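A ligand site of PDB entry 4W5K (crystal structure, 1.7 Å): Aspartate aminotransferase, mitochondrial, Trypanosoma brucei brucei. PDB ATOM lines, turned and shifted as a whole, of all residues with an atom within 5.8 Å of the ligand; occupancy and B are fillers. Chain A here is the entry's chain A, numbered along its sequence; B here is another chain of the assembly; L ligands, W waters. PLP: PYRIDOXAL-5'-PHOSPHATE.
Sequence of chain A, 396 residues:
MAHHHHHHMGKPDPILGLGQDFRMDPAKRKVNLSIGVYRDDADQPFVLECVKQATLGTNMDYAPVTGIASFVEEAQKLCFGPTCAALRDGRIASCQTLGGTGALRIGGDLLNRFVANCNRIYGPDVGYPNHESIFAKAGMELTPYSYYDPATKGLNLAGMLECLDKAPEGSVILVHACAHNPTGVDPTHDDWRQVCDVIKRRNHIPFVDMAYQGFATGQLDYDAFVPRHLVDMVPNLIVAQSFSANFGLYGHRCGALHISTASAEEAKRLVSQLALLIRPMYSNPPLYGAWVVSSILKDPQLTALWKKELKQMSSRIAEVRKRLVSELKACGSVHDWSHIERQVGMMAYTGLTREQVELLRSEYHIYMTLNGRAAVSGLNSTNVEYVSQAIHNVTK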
ATOM      1  N   GLY A  36     -20.079  36.030   8.970  1.00  0.00           N
ATOM      2  CA  GLY A  36     -18.729  35.501   8.861  1.00  0.00           C
ATOM      3  C   GLY A  36     -18.622  34.305   7.934  1.00  0.00           C
ATOM      4  O   GLY A  36     -17.547  33.726   7.806  1.00  0.00           O
ATOM      5  N   LEU A  98      -8.677  21.567  15.073  1.00  0.00           N
ATOM      6  CA  LEU A  98     -10.035  22.094  15.153  1.00  0.00           C
ATOM      7  C   LEU A  98     -10.156  23.363  14.316  1.00  0.00           C
ATOM      8  O   LEU A  98     -10.087  24.484  14.854  1.00  0.00           O
ATOM      9  CB  LEU A  98     -10.380  22.377  16.617  1.00  0.00           C
ATOM     10  CG  LEU A  98     -10.345  21.120  17.485  1.00  0.00           C
ATOM     11  CD1 LEU A  98     -10.477  21.455  18.953  1.00  0.00           C
ATOM     12  CD2 LEU A  98     -11.492  20.253  17.024  1.00  0.00           C
ATOM     13  N   GLY A  99     -10.348  23.176  13.008  1.00  0.00           N
ATOM     14  CA  GLY A  99     -10.311  24.272  12.059  1.00  0.00           C
ATOM     15  C   GLY A  99      -8.968  24.986  11.990  1.00  0.00           C
ATOM     16  O   GLY A  99      -7.964  24.546  12.562  1.00  0.00           O
ATOM     17  N   GLY A 100      -8.924  26.087  11.257  1.00  0.00           N
ATOM     18  CA  GLY A 100      -7.731  26.916  11.270  1.00  0.00           C
ATOM     19  C   GLY A 100      -7.409  27.483  12.643  1.00  0.00           C
ATOM     20  O   GLY A 100      -6.210  27.717  12.966  1.00  0.00           O
ATOM     21  N   THR A 101      -8.449  27.707  13.454  1.00  0.00           N
ATOM     22  CA  THR A 101      -8.246  28.257  14.799  1.00  0.00           C
ATOM     23  C   THR A 101      -7.412  27.302  15.624  1.00  0.00           C
ATOM     24  O   THR A 101      -6.431  27.729  16.240  1.00  0.00           O
ATOM     25  CB  THR A 101      -9.568  28.542  15.522  1.00  0.00           C
ATOM     26  OG1 THR A 101     -10.382  29.430  14.717  1.00  0.00           O
ATOM     27  CG2 THR A 101      -9.306  29.173  16.891  1.00  0.00           C
ATOM     28  N   GLY A 102      -7.799  26.026  15.608  1.00  0.00           N
ATOM     29  CA  GLY A 102      -7.026  25.001  16.339  1.00  0.00           C
ATOM     30  C   GLY A 102      -5.576  24.932  15.846  1.00  0.00           C
ATOM     31  O   GLY A 102      -4.626  24.792  16.648  1.00  0.00           O
ATOM     32  N   LEU A 104      -3.811  27.396  14.528  1.00  0.00           N
ATOM     33  CA  LEU A 104      -3.117  28.587  15.038  1.00  0.00           C
ATOM     34  C   LEU A 104      -2.718  28.407  16.494  1.00  0.00           C
ATOM     35  O   LEU A 104      -1.610  28.755  16.896  1.00  0.00           O
ATOM     36  CB  LEU A 104      -3.996  29.831  14.897  1.00  0.00           C
ATOM     37  CG  LEU A 104      -4.149  30.223  13.429  1.00  0.00           C
ATOM     38  CD1 LEU A 104      -5.383  31.088  13.261  1.00  0.00           C
ATOM     39  CD2 LEU A 104      -2.848  30.965  12.917  1.00  0.00           C
ATOM     40  N   TYR A 128      -6.878  39.836  11.972  1.00  0.00           N
ATOM     41  CA  TYR A 128      -7.959  39.008  12.432  1.00  0.00           C
ATOM     42  C   TYR A 128      -8.051  39.075  13.963  1.00  0.00           C
ATOM     43  O   TYR A 128      -7.079  38.775  14.665  1.00  0.00           O
ATOM     44  CB  TYR A 128      -7.682  37.591  11.930  1.00  0.00           C
ATOM     45  CG  TYR A 128      -8.680  36.549  12.290  1.00  0.00           C
ATOM     46  CD1 TYR A 128      -9.975  36.598  11.799  1.00  0.00           C
ATOM     47  CD2 TYR A 128      -8.291  35.459  13.068  1.00  0.00           C
ATOM     48  CE1 TYR A 128     -10.902  35.582  12.139  1.00  0.00           C
ATOM     49  CE2 TYR A 128      -9.191  34.458  13.392  1.00  0.00           C
ATOM     50  CZ  TYR A 128     -10.487  34.526  12.918  1.00  0.00           C
ATOM     51  OH  TYR A 128     -11.374  33.524  13.238  1.00  0.00           O
ATOM     52  N   HIS A 131      -6.647  36.503  16.533  1.00  0.00           N
ATOM     53  CA  HIS A 131      -5.227  36.179  16.521  1.00  0.00           C
ATOM     54  C   HIS A 131      -4.558  36.643  17.801  1.00  0.00           C
ATOM     55  O   HIS A 131      -3.695  35.956  18.352  1.00  0.00           O
ATOM     56  CB  HIS A 131      -4.515  36.817  15.304  1.00  0.00           C
ATOM     57  CG  HIS A 131      -4.593  35.997  14.062  1.00  0.00           C
ATOM     58  ND1 HIS A 131      -4.481  36.555  12.805  1.00  0.00           N
ATOM     59  CD2 HIS A 131      -4.740  34.663  13.868  1.00  0.00           C
ATOM     60  CE1 HIS A 131      -4.573  35.607  11.893  1.00  0.00           C
ATOM     61  NE2 HIS A 131      -4.728  34.446  12.510  1.00  0.00           N
ATOM     62  N   HIS A 176      -1.299  36.425   6.232  1.00  0.00           N
ATOM     63  CA  HIS A 176      -2.501  35.775   5.673  1.00  0.00           C
ATOM     64  C   HIS A 176      -2.173  35.329   4.239  1.00  0.00           C
ATOM     65  O   HIS A 176      -1.664  36.141   3.459  1.00  0.00           O
ATOM     66  CB  HIS A 176      -3.712  36.730   5.642  1.00  0.00           C
ATOM     67  CG  HIS A 176      -4.140  37.259   6.977  1.00  0.00           C
ATOM     68  ND1 HIS A 176      -5.477  37.418   7.307  1.00  0.00           N
ATOM     69  CD2 HIS A 176      -3.427  37.680   8.051  1.00  0.00           C
ATOM     70  CE1 HIS A 176      -5.555  37.923   8.527  1.00  0.00           C
ATOM     71  NE2 HIS A 176      -4.335  38.089   9.008  1.00  0.00           N
ATOM     72  N   ALA A 179      -7.027  36.432   0.697  1.00  0.00           N
ATOM     73  CA  ALA A 179      -8.248  36.958   1.293  1.00  0.00           C
ATOM     74  C   ALA A 179      -8.013  37.415   2.740  1.00  0.00           C
ATOM     75  O   ALA A 179      -8.653  36.941   3.696  1.00  0.00           O
ATOM     76  CB  ALA A 179      -9.417  35.916   1.205  1.00  0.00           C
ATOM     77  N   ASN A 181      -8.292  38.887   6.136  1.00  0.00           N
ATOM     78  CA  ASN A 181      -9.460  39.173   6.966  1.00  0.00           C
ATOM     79  C   ASN A 181      -8.970  40.124   8.046  1.00  0.00           C
ATOM     80  O   ASN A 181      -8.111  39.769   8.868  1.00  0.00           O
ATOM     81  CB  ASN A 181     -10.031  37.838   7.524  1.00  0.00           C
ATOM     82  CG  ASN A 181     -11.277  38.014   8.408  1.00  0.00           C
ATOM     83  OD1 ASN A 181     -11.660  39.128   8.773  1.00  0.00           O
ATOM     84  ND2 ASN A 181     -11.870  36.897   8.774  1.00  0.00           N
ATOM     85  N   ASP A 209      -1.267  31.887   7.925  1.00  0.00           N
ATOM     86  CA  ASP A 209      -2.677  31.587   8.162  1.00  0.00           C
ATOM     87  C   ASP A 209      -3.336  31.485   6.780  1.00  0.00           C
ATOM     88  O   ASP A 209      -3.499  32.486   6.081  1.00  0.00           O
ATOM     89  CB  ASP A 209      -3.337  32.676   9.038  1.00  0.00           C
ATOM     90  CG  ASP A 209      -4.799  32.380   9.355  1.00  0.00           C
ATOM     91  OD1 ASP A 209      -5.394  31.494   8.712  1.00  0.00           O
ATOM     92  OD2 ASP A 209      -5.371  33.032  10.264  1.00  0.00           O
ATOM     93  N   ALA A 211      -6.605  30.462   5.431  1.00  0.00           N
ATOM     94  CA  ALA A 211      -7.988  30.108   5.761  1.00  0.00           C
ATOM     95  C   ALA A 211      -8.866  29.995   4.528  1.00  0.00           C
ATOM     96  O   ALA A 211      -9.992  29.516   4.657  1.00  0.00           O
ATOM     97  CB  ALA A 211      -8.583  31.167   6.754  1.00  0.00           C
ATOM     98  N   TYR A 212      -8.392  30.424   3.352  1.00  0.00           N
ATOM     99  CA  TYR A 212      -9.267  30.531   2.181  1.00  0.00           C
ATOM    100  C   TYR A 212      -8.636  30.008   0.894  1.00  0.00           C
ATOM    101  O   TYR A 212      -8.927  30.544  -0.158  1.00  0.00           O
ATOM    102  CB  TYR A 212      -9.692  31.999   1.974  1.00  0.00           C
ATOM    103  CG  TYR A 212     -10.391  32.571   3.185  1.00  0.00           C
ATOM    104  CD1 TYR A 212     -11.706  32.236   3.458  1.00  0.00           C
ATOM    105  CD2 TYR A 212      -9.722  33.448   4.055  1.00  0.00           C
ATOM    106  CE1 TYR A 212     -12.367  32.726   4.566  1.00  0.00           C
ATOM    107  CE2 TYR A 212     -10.366  33.953   5.192  1.00  0.00           C
ATOM    108  CZ  TYR A 212     -11.696  33.566   5.430  1.00  0.00           C
ATOM    109  OH  TYR A 212     -12.361  34.041   6.530  1.00  0.00           O
ATOM    110  N   SER A 242      -7.340  26.005   7.058  1.00  0.00           N
ATOM    111  CA  SER A 242      -8.761  25.839   7.363  1.00  0.00           C
ATOM    112  C   SER A 242      -9.554  25.229   6.203  1.00  0.00           C
ATOM    113  O   SER A 242      -9.388  25.624   5.042  1.00  0.00           O
ATOM    114  CB  SER A 242      -9.382  27.194   7.734  1.00  0.00           C
ATOM    115  OG  SER A 242     -10.801  27.068   7.895  1.00  0.00           O
ATOM    116  N   PHE A 243     -10.439  24.287   6.533  1.00  0.00           N
ATOM    117  CA  PHE A 243     -11.374  23.751   5.554  1.00  0.00           C
ATOM    118  C   PHE A 243     -12.784  24.274   5.744  1.00  0.00           C
ATOM    119  O   PHE A 243     -13.722  23.814   5.080  1.00  0.00           O
ATOM    120  CB  PHE A 243     -11.322  22.217   5.601  1.00  0.00           C
ATOM    121  CG  PHE A 243      -9.994  21.683   5.164  1.00  0.00           C
ATOM    122  CD1 PHE A 243      -9.556  21.872   3.864  1.00  0.00           C
ATOM    123  CD2 PHE A 243      -9.128  21.102   6.072  1.00  0.00           C
ATOM    124  CE1 PHE A 243      -8.295  21.433   3.467  1.00  0.00           C
ATOM    125  CE2 PHE A 243      -7.870  20.639   5.671  1.00  0.00           C
ATOM    126  CZ  PHE A 243      -7.459  20.804   4.366  1.00  0.00           C
ATOM    127  N   SER A 244     -12.922  25.297   6.593  1.00  0.00           N
ATOM    128  CA  SER A 244     -14.242  25.833   6.895  1.00  0.00           C
ATOM    129  C   SER A 244     -14.893  26.506   5.709  1.00  0.00           C
ATOM    130  O   SER A 244     -16.009  26.156   5.327  1.00  0.00           O
ATOM    131  CB  SER A 244     -14.163  26.821   8.071  1.00  0.00           C
ATOM    132  OG  SER A 244     -13.798  26.124   9.269  1.00  0.00           O
ATOM    133  N   TYR A 250     -17.607  24.845   8.064  1.00  0.00           N
ATOM    134  CA  TYR A 250     -17.461  25.711   9.237  1.00  0.00           C
ATOM    135  C   TYR A 250     -17.666  25.047  10.601  1.00  0.00           C
ATOM    136  O   TYR A 250     -16.700  24.859  11.372  1.00  0.00           O
ATOM    137  CB  TYR A 250     -18.454  26.882   9.112  1.00  0.00           C
ATOM    138  CG  TYR A 250     -18.333  27.689   7.819  1.00  0.00           C
ATOM    139  CD1 TYR A 250     -17.390  28.705   7.704  1.00  0.00           C
ATOM    140  CD2 TYR A 250     -19.188  27.455   6.746  1.00  0.00           C
ATOM    141  CE1 TYR A 250     -17.275  29.455   6.522  1.00  0.00           C
ATOM    142  CE2 TYR A 250     -19.091  28.220   5.572  1.00  0.00           C
ATOM    143  CZ  TYR A 250     -18.134  29.198   5.471  1.00  0.00           C
ATOM    144  OH  TYR A 250     -18.037  29.946   4.330  1.00  0.00           O
ATOM    145  N   ARG A 253     -15.598  21.897  12.245  1.00  0.00           N
ATOM    146  CA  ARG A 253     -14.294  22.214  12.847  1.00  0.00           C
ATOM    147  C   ARG A 253     -13.169  21.370  12.267  1.00  0.00           C
ATOM    148  O   ARG A 253     -12.568  20.527  12.970  1.00  0.00           O
ATOM    149  CB  ARG A 253     -14.331  22.044  14.371  1.00  0.00           C
ATOM    150  CG  ARG A 253     -15.538  22.711  15.073  1.00  0.00           C
ATOM    151  CD  ARG A 253     -15.763  24.176  14.598  1.00  0.00           C
ATOM    152  NE  ARG A 253     -14.641  25.052  14.963  1.00  0.00           N
ATOM    153  CZ  ARG A 253     -13.923  25.761  14.095  1.00  0.00           C
ATOM    154  NH1 ARG A 253     -14.188  25.717  12.789  1.00  0.00           N
ATOM    155  NH2 ARG A 253     -12.924  26.517  14.542  1.00  0.00           N
ATOM    156  N   CYS A 254     -12.856  21.636  10.992  1.00  0.00           N
ATOM    157  CA  CYS A 254     -11.933  20.819  10.250  1.00  0.00           C
ATOM    158  C   CYS A 254     -10.798  21.695   9.725  1.00  0.00           C
ATOM    159  O   CYS A 254     -11.048  22.655   8.991  1.00  0.00           O
ATOM    160  CB  CYS A 254     -12.646  20.141   9.082  1.00  0.00           C
ATOM    161  SG  CYS A 254     -11.642  19.032   8.122  1.00  0.00           S
ATOM    162  N   TYR B  62     -21.236  27.894  11.770  1.00  0.00           N
ATOM    163  CA  TYR B  62     -20.675  27.777  13.119  1.00  0.00           C
ATOM    164  C   TYR B  62     -21.732  27.759  14.211  1.00  0.00           C
ATOM    165  O   TYR B  62     -22.702  28.533  14.161  1.00  0.00           O
ATOM    166  CB  TYR B  62     -19.742  28.953  13.403  1.00  0.00           C
ATOM    167  CG  TYR B  62     -18.531  29.078  12.545  1.00  0.00           C
ATOM    168  CD1 TYR B  62     -17.486  28.179  12.675  1.00  0.00           C
ATOM    169  CD2 TYR B  62     -18.392  30.151  11.656  1.00  0.00           C
ATOM    170  CE1 TYR B  62     -16.346  28.331  11.899  1.00  0.00           C
ATOM    171  CE2 TYR B  62     -17.256  30.307  10.888  1.00  0.00           C
ATOM    172  CZ  TYR B  62     -16.239  29.392  11.035  1.00  0.00           C
ATOM    173  OH  TYR B  62     -15.086  29.554  10.300  1.00  0.00           O
ATOM    174  N   TYR B 282     -10.308  26.992  20.049  1.00  0.00           N
ATOM    175  CA  TYR B 282     -10.870  26.359  18.851  1.00  0.00           C
ATOM    176  C   TYR B 282     -12.084  27.099  18.288  1.00  0.00           C
ATOM    177  O   TYR B 282     -12.771  26.563  17.410  1.00  0.00           O
ATOM    178  CB  TYR B 282     -11.231  24.891  19.146  1.00  0.00           C
ATOM    179  CG  TYR B 282     -12.184  24.716  20.299  1.00  0.00           C
ATOM    180  CD1 TYR B 282     -13.562  24.804  20.120  1.00  0.00           C
ATOM    181  CD2 TYR B 282     -11.695  24.432  21.582  1.00  0.00           C
ATOM    182  CE1 TYR B 282     -14.450  24.624  21.190  1.00  0.00           C
ATOM    183  CE2 TYR B 282     -12.566  24.274  22.652  1.00  0.00           C
ATOM    184  CZ  TYR B 282     -13.934  24.372  22.448  1.00  0.00           C
ATOM    185  OH  TYR B 282     -14.779  24.222  23.531  1.00  0.00           O
ATOM    186  N   SER B 283     -12.340  28.297  18.818  1.00  0.00           N
ATOM    187  CA  SER B 283     -13.375  29.212  18.332  1.00  0.00           C
ATOM    188  C   SER B 283     -14.815  28.785  18.698  1.00  0.00           C
ATOM    189  O   SER B 283     -15.554  29.533  19.359  1.00  0.00           O
ATOM    190  CB  SER B 283     -13.257  29.383  16.805  1.00  0.00           C
ATOM    191  OG  SER B 283     -13.954  30.531  16.367  1.00  0.00           O
HETATM  192  N1  PLP L   1      -7.963  32.779  10.296  1.00  0.00           N
HETATM  193  C2  PLP L   1      -8.659  33.640   9.475  1.00  0.00           C
HETATM  194  C2A PLP L   1      -7.906  34.694   8.744  1.00  0.00           C
HETATM  195  C3  PLP L   1     -10.043  33.520   9.351  1.00  0.00           C
HETATM  196  O3  PLP L   1     -10.763  34.372   8.558  1.00  0.00           O
HETATM  197  C4  PLP L   1     -10.722  32.524  10.037  1.00  0.00           C
HETATM  198  C4A PLP L   1     -12.161  32.277   9.699  1.00  0.00           C
HETATM  199  O4A PLP L   1     -13.016  33.047  10.139  1.00  0.00           O
HETATM  200  C5  PLP L   1     -10.011  31.653  10.859  1.00  0.00           C
HETATM  201  C6  PLP L   1      -8.623  31.777  10.971  1.00  0.00           C
HETATM  202  C5A PLP L   1     -10.729  30.563  11.654  1.00  0.00           C
HETATM  203  O4P PLP L   1     -11.092  29.501  10.819  1.00  0.00           O
HETATM  204  P   PLP L   1     -11.723  28.193  11.390  1.00  0.00           P
HETATM  205  O1P PLP L   1     -13.223  28.296  11.407  1.00  0.00           O
HETATM  206  O2P PLP L   1     -11.197  27.926  12.775  1.00  0.00           O
HETATM  207  O3P PLP L   1     -11.275  27.113  10.429  1.00  0.00           O
HETATM  208  O   HOH W   1     -14.108  30.335  13.467  1.00  0.00           O
HETATM  209  O   HOH W   2     -14.380  36.184   9.730  1.00  0.00           O
HETATM  210  O   HOH W   3     -14.361  30.672   7.511  1.00  0.00           O
HETATM  211  O   HOH W   4      -7.269  35.575   5.748  1.00  0.00           O
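Gly 99 touches the ligand. Tyr 128 touches the ligand. His 176 touches the ligand. CB of Ala 211 touches C2 of the ligand, at 3.7 Å. Hydrophobic or aromatic side chains within 4 Å of the ligand: Tyr 128, Ala 211, Tyr 212 and Tyr 62 of chain B. Within 4 Å of the ligand: Gly 99, Gly 100, Thr 101, Tyr 128, His 176, Asn 181, Asp 209, Ala 211, Tyr 212, Ser 242, Ser 244, Arg 253 and Tyr 62 of chain B.
OH of Tyr 62 of chain B lies within hydrogen-bond range of O1P of the ligand. The side-chain hydroxyl (OG) of Ser 242 sits at hydrogen-bond distance from an oxygen (O3P) of the ligand (2.6 Å). The backbone NH (N) of Thr 101 is in hydrogen-bond range of an oxygen (O2P) of the ligand, at 2.8 Å. OG1 of Thr 101 sits at hydrogen-bond distance from O2P of the ligand, 2.6 Å away. OH of Tyr 212 lies within hydrogen-bond range of O3 of the ligand (2.6 Å). A nitrogen (N1) of the ligand sits at hydrogen-bond distance from the side-chain carboxylate (OD2) of Asp 209, at 2.6 Å. An oxygen (O3P) of the ligand sits at hydrogen-bond distance from the backbone NH (N) of Gly 100 (2.7 Å). The side-chain amide nitrogen (ND2) of Asn 181 lies within hydrogen-bond range of an oxygen (O3) of the ligand (2.8 Å). NH2 of Arg 253 lies within salt-bridge range of O2P of the ligand (2.8 Å). The side-chain hydroxyl of Ser 244 sits at hydrogen-bond distance from an oxygen (O3P) of the ligand.
Water W1 lies within hydrogen-bond range of OG of Ser 283 of chain B, O1P of the ligand and OH of Tyr 62 of chain B. Water W4 lies within hydrogen-bond range of the backbone carbonyl oxygen (O) of Ala 179, a ring nitrogen (ND1) of His 176 and the backbone NH (N) of Asn 181. Water W2 bridges ND2 of Asn 181 (2.8 Å) and O4A of the ligand (3.4 Å).
The side-chain hydroxyl (OG) of Ser 242 sits at hydrogen-bond distance from the backbone NH (N) of Ser 244, at 3.1 Å. OD2 of Asp 209 lies within hydrogen-bond range of NE2 of His 131 (2.7 Å). The backbone NH of Tyr 128 sits at hydrogen-bond distance from the backbone carbonyl oxygen of Asn 181 (3.3 Å). N of Asn 181 lies within hydrogen-bond range of ND1 of His 176. N of Gly 99 lies close to O of Arg 253, 3.5 Å away. The backbone carbonyl oxygen (O) of Tyr 250 lies within hydrogen-bond range of the guanidinium group (NH1) of Arg 253. NH2 of Arg 253 lies within hydrogen-bond range of O of Tyr 282 of chain B, at 2.9 Å. N of Tyr 250 sits at hydrogen-bond distance from O of Ser 244 (3.4 Å).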
